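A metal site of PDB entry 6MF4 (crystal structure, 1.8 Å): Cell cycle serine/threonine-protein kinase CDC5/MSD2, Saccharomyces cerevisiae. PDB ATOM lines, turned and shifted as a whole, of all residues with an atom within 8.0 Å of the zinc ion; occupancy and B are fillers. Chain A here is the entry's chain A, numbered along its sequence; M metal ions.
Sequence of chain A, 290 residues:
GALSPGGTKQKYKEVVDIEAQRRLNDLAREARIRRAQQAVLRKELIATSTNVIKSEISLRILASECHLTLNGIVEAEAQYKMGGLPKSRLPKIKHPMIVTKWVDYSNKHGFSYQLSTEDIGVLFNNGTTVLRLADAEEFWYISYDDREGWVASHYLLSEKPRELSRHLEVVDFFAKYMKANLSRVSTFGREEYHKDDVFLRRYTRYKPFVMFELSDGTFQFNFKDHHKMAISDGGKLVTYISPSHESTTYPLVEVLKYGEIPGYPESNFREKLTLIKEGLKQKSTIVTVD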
ATOM      1  N   LEU A 133     -14.427  -1.757   7.417  1.00  0.00           N
ATOM      2  CA  LEU A 133     -15.108  -2.787   6.636  1.00  0.00           C
ATOM      3  C   LEU A 133     -14.818  -4.160   7.205  1.00  0.00           C
ATOM      4  O   LEU A 133     -13.806  -4.392   7.858  1.00  0.00           O
ATOM      5  CB  LEU A 133     -14.690  -2.725   5.169  1.00  0.00           C
ATOM      6  CG  LEU A 133     -15.481  -1.729   4.317  1.00  0.00           C
ATOM      7  CD1 LEU A 133     -15.031  -0.317   4.602  1.00  0.00           C
ATOM      8  CD2 LEU A 133     -15.357  -2.039   2.837  1.00  0.00           C
ATOM      9  N   ASP A 135     -13.849  -6.708   5.894  1.00  0.00           N
ATOM     10  CA  ASP A 135     -12.699  -7.395   5.327  1.00  0.00           C
ATOM     11  C   ASP A 135     -11.436  -7.180   6.169  1.00  0.00           C
ATOM     12  O   ASP A 135     -10.411  -7.823   5.941  1.00  0.00           O
ATOM     13  CB  ASP A 135     -12.455  -6.941   3.879  1.00  0.00           C
ATOM     14  CG  ASP A 135     -12.283  -5.429   3.744  1.00  0.00           C
ATOM     15  OD1 ASP A 135     -11.831  -4.770   4.700  1.00  0.00           O
ATOM     16  OD2 ASP A 135     -12.569  -4.911   2.645  1.00  0.00           O
ATOM     17  N   GLU A 137      -9.404  -4.826   6.123  1.00  0.00           N
ATOM     18  CA  GLU A 137      -8.313  -4.212   5.375  1.00  0.00           C
ATOM     19  C   GLU A 137      -8.606  -2.773   4.943  1.00  0.00           C
ATOM     20  O   GLU A 137      -7.689  -1.964   4.803  1.00  0.00           O
ATOM     21  CB  GLU A 137      -7.972  -5.060   4.127  1.00  0.00           C
ATOM     22  CG  GLU A 137      -7.076  -4.375   3.076  1.00  0.00           C
ATOM     23  CD  GLU A 137      -5.745  -3.858   3.621  1.00  0.00           C
ATOM     24  OE1 GLU A 137      -4.991  -3.250   2.836  1.00  0.00           O
ATOM     25  OE2 GLU A 137      -5.439  -4.052   4.820  1.00  0.00           O
ATOM     26  N   GLU A 138      -9.888  -2.456   4.728  1.00  0.00           N
ATOM     27  CA  GLU A 138     -10.269  -1.117   4.294  1.00  0.00           C
ATOM     28  C   GLU A 138     -11.104  -0.399   5.348  1.00  0.00           C
ATOM     29  O   GLU A 138     -11.839  -1.027   6.099  1.00  0.00           O
ATOM     30  CB  GLU A 138     -11.051  -1.176   2.980  1.00  0.00           C
ATOM     31  CG  GLU A 138     -10.333  -1.898   1.850  1.00  0.00           C
ATOM     32  CD  GLU A 138     -10.799  -1.436   0.485  1.00  0.00           C
ATOM     33  OE1 GLU A 138     -11.992  -1.129   0.326  1.00  0.00           O
ATOM     34  OE2 GLU A 138      -9.958  -1.374  -0.437  1.00  0.00           O
ATOM     35  N   PHE A 139     -10.990   0.932   5.386  1.00  0.00           N
ATOM     36  CA  PHE A 139     -11.881   1.730   6.214  1.00  0.00           C
ATOM     37  C   PHE A 139     -12.136   3.092   5.590  1.00  0.00           C
ATOM     38  O   PHE A 139     -11.361   3.571   4.757  1.00  0.00           O
ATOM     39  CB  PHE A 139     -11.334   1.883   7.651  1.00  0.00           C
ATOM     40  CG  PHE A 139     -10.137   2.794   7.773  1.00  0.00           C
ATOM     41  CD1 PHE A 139      -8.848   2.293   7.630  1.00  0.00           C
ATOM     42  CD2 PHE A 139     -10.292   4.138   8.070  1.00  0.00           C
ATOM     43  CE1 PHE A 139      -7.743   3.121   7.764  1.00  0.00           C
ATOM     44  CE2 PHE A 139      -9.196   4.968   8.207  1.00  0.00           C
ATOM     45  CZ  PHE A 139      -7.915   4.464   8.037  1.00  0.00           C
ATOM     46  N   TRP A 140     -13.269   3.678   5.975  1.00  0.00           N
ATOM     47  CA  TRP A 140     -13.611   5.062   5.651  1.00  0.00           C
ATOM     48  C   TRP A 140     -13.391   5.951   6.859  1.00  0.00           C
ATOM     49  O   TRP A 140     -13.786   5.594   7.966  1.00  0.00           O
ATOM     50  CB  TRP A 140     -15.075   5.186   5.227  1.00  0.00           C
ATOM     51  CG  TRP A 140     -15.452   4.486   3.969  1.00  0.00           C
ATOM     52  CD1 TRP A 140     -16.092   3.287   3.872  1.00  0.00           C
ATOM     53  CD2 TRP A 140     -15.255   4.958   2.639  1.00  0.00           C
ATOM     54  NE1 TRP A 140     -16.300   2.971   2.554  1.00  0.00           N
ATOM     55  CE2 TRP A 140     -15.787   3.982   1.770  1.00  0.00           C
ATOM     56  CE3 TRP A 140     -14.669   6.095   2.082  1.00  0.00           C
ATOM     57  CZ2 TRP A 140     -15.756   4.106   0.386  1.00  0.00           C
ATOM     58  CZ3 TRP A 140     -14.646   6.228   0.707  1.00  0.00           C
ATOM     59  CH2 TRP A 140     -15.189   5.243  -0.127  1.00  0.00           C
ATOM     60  N   HIS A 154     -11.311   7.187   1.649  1.00  0.00           N
ATOM     61  CA  HIS A 154     -11.002   5.758   1.557  1.00  0.00           C
ATOM     62  C   HIS A 154      -9.561   5.471   1.980  1.00  0.00           C
ATOM     63  O   HIS A 154      -8.632   6.061   1.439  1.00  0.00           O
ATOM     64  CB  HIS A 154     -11.254   5.303   0.114  1.00  0.00           C
ATOM     65  CG  HIS A 154     -11.028   3.843  -0.136  1.00  0.00           C
ATOM     66  ND1 HIS A 154      -9.783   3.266  -0.110  1.00  0.00           N
ATOM     67  CD2 HIS A 154     -11.895   2.855  -0.463  1.00  0.00           C
ATOM     68  CE1 HIS A 154      -9.890   1.978  -0.392  1.00  0.00           C
ATOM     69  NE2 HIS A 154     -11.159   1.705  -0.620  1.00  0.00           N
ATOM     70  N   TYR A 155      -9.375   4.562   2.949  1.00  0.00           N
ATOM     71  CA  TYR A 155      -8.040   4.176   3.413  1.00  0.00           C
ATOM     72  C   TYR A 155      -7.863   2.665   3.553  1.00  0.00           C
ATOM     73  O   TYR A 155      -8.840   1.921   3.639  1.00  0.00           O
ATOM     74  CB  TYR A 155      -7.737   4.816   4.764  1.00  0.00           C
ATOM     75  CG  TYR A 155      -7.526   6.311   4.700  1.00  0.00           C
ATOM     76  CD1 TYR A 155      -6.356   6.844   4.187  1.00  0.00           C
ATOM     77  CD2 TYR A 155      -8.501   7.177   5.176  1.00  0.00           C
ATOM     78  CE1 TYR A 155      -6.170   8.207   4.134  1.00  0.00           C
ATOM     79  CE2 TYR A 155      -8.315   8.540   5.123  1.00  0.00           C
ATOM     80  CZ  TYR A 155      -7.149   9.052   4.606  1.00  0.00           C
ATOM     81  OH  TYR A 155      -6.972  10.416   4.556  1.00  0.00           O
ATOM     82  N   LEU A 156      -6.599   2.243   3.574  1.00  0.00           N
ATOM     83  CA  LEU A 156      -6.233   0.871   3.904  1.00  0.00           C
ATOM     84  C   LEU A 156      -5.608   0.833   5.297  1.00  0.00           C
ATOM     85  O   LEU A 156      -4.806   1.707   5.631  1.00  0.00           O
ATOM     86  CB  LEU A 156      -5.242   0.312   2.878  1.00  0.00           C
ATOM     87  CG  LEU A 156      -5.617   0.431   1.403  1.00  0.00           C
ATOM     88  CD1 LEU A 156      -4.522  -0.177   0.542  1.00  0.00           C
ATOM     89  CD2 LEU A 156      -6.955  -0.255   1.127  1.00  0.00           C
ATOM     90  N   PHE A 188     -19.969   7.441  -0.547  1.00  0.00           N
ATOM     91  CA  PHE A 188     -18.958   6.393  -0.707  1.00  0.00           C
ATOM     92  C   PHE A 188     -18.659   6.017  -2.168  1.00  0.00           C
ATOM     93  O   PHE A 188     -18.052   4.977  -2.422  1.00  0.00           O
ATOM     94  CB  PHE A 188     -19.393   5.143   0.057  1.00  0.00           C
ATOM     95  CG  PHE A 188     -19.634   5.392   1.519  1.00  0.00           C
ATOM     96  CD1 PHE A 188     -18.582   5.664   2.369  1.00  0.00           C
ATOM     97  CD2 PHE A 188     -20.910   5.333   2.031  1.00  0.00           C
ATOM     98  CE1 PHE A 188     -18.809   5.897   3.709  1.00  0.00           C
ATOM     99  CE2 PHE A 188     -21.148   5.554   3.376  1.00  0.00           C
ATOM    100  CZ  PHE A 188     -20.086   5.845   4.214  1.00  0.00           C
ATOM    101  N   GLU A 191     -18.040   2.615  -6.861  1.00  0.00           N
ATOM    102  CA  GLU A 191     -17.318   1.353  -7.019  1.00  0.00           C
ATOM    103  C   GLU A 191     -18.201   0.212  -6.505  1.00  0.00           C
ATOM    104  O   GLU A 191     -18.943   0.396  -5.538  1.00  0.00           O
ATOM    105  CB  GLU A 191     -15.983   1.384  -6.279  1.00  0.00           C
ATOM    106  CG  GLU A 191     -14.782   1.752  -7.151  1.00  0.00           C
ATOM    107  CD  GLU A 191     -14.179   0.541  -7.841  1.00  0.00           C
ATOM    108  OE1 GLU A 191     -13.531  -0.282  -7.160  1.00  0.00           O
ATOM    109  OE2 GLU A 191     -14.349   0.409  -9.075  1.00  0.00           O
ATOM    110  N   TYR A 193     -17.656  -2.462  -4.837  1.00  0.00           N
ATOM    111  CA  TYR A 193     -17.382  -2.927  -3.479  1.00  0.00           C
ATOM    112  C   TYR A 193     -17.954  -1.997  -2.412  1.00  0.00           C
ATOM    113  O   TYR A 193     -18.076  -2.403  -1.250  1.00  0.00           O
ATOM    114  CB  TYR A 193     -15.863  -3.056  -3.294  1.00  0.00           C
ATOM    115  CG  TYR A 193     -15.407  -3.919  -2.136  1.00  0.00           C
ATOM    116  CD1 TYR A 193     -15.655  -5.287  -2.116  1.00  0.00           C
ATOM    117  CD2 TYR A 193     -14.669  -3.372  -1.087  1.00  0.00           C
ATOM    118  CE1 TYR A 193     -15.222  -6.082  -1.068  1.00  0.00           C
ATOM    119  CE2 TYR A 193     -14.223  -4.161  -0.036  1.00  0.00           C
ATOM    120  CZ  TYR A 193     -14.498  -5.514  -0.039  1.00  0.00           C
ATOM    121  OH  TYR A 193     -14.073  -6.294   1.010  1.00  0.00           O
ATOM    122  N   HIS A 194     -18.329  -0.782  -2.808  1.00  0.00           N
ATOM    123  CA  HIS A 194     -18.707   0.266  -1.847  1.00  0.00           C
ATOM    124  C   HIS A 194     -20.090   0.864  -2.069  1.00  0.00           C
ATOM    125  O   HIS A 194     -20.532   1.686  -1.262  1.00  0.00           O
ATOM    126  CB  HIS A 194     -17.676   1.390  -1.885  1.00  0.00           C
ATOM    127  CG  HIS A 194     -16.335   0.995  -1.363  1.00  0.00           C
ATOM    128  ND1 HIS A 194     -16.147   0.530  -0.083  1.00  0.00           N
ATOM    129  CD2 HIS A 194     -15.114   0.978  -1.956  1.00  0.00           C
ATOM    130  CE1 HIS A 194     -14.870   0.253   0.100  1.00  0.00           C
ATOM    131  NE2 HIS A 194     -14.219   0.517  -1.025  1.00  0.00           N
ATOM    132  N   ASP A 197     -22.455   0.867   0.788  1.00  0.00           N
ATOM    133  CA  ASP A 197     -21.862   1.207   2.083  1.00  0.00           C
ATOM    134  C   ASP A 197     -22.761   2.183   2.839  1.00  0.00           C
ATOM    135  O   ASP A 197     -23.365   3.069   2.243  1.00  0.00           O
ATOM    136  CB  ASP A 197     -20.458   1.799   1.910  1.00  0.00           C
ATOM    137  CG  ASP A 197     -19.410   0.743   1.590  1.00  0.00           C
ATOM    138  OD1 ASP A 197     -19.783  -0.424   1.313  1.00  0.00           O
ATOM    139  OD2 ASP A 197     -18.202   1.078   1.617  1.00  0.00           O
HETATM  140 ZN    ZN M   1     -12.283   0.058  -1.236  1.00  0.00          ZN
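A ring nitrogen (ND1) of His 194 lies within hydrogen-bond range of the side-chain carboxylate (OD2) of Asp 197 (2.7 Å). N of Glu 138 sits at hydrogen-bond distance from OD1 of Asp 135. The backbone carbonyl oxygen (O) of Glu 138 lies within hydrogen-bond range of the backbone NH (N) of Leu 133 (3.0 Å).
Within 4 Å of the zinc ion: Glu 138, His 154 and His 194. The nearest printed residue that does not touch the zinc ion is Tyr 193 (4.2 Å).
The zinc ion is bound by the side-chain carboxylate of Glu 138 (2.0 Å), a ring nitrogen (NE2) of His 194 (2.0 Å) and a ring nitrogen (NE2) of His 154 (2.1 Å). The zinc ion has three donor atoms within binding distance. Slightly farther from the zinc ion lies the side-chain carboxylate (OE2) of Glu 138 (2.8 Å).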
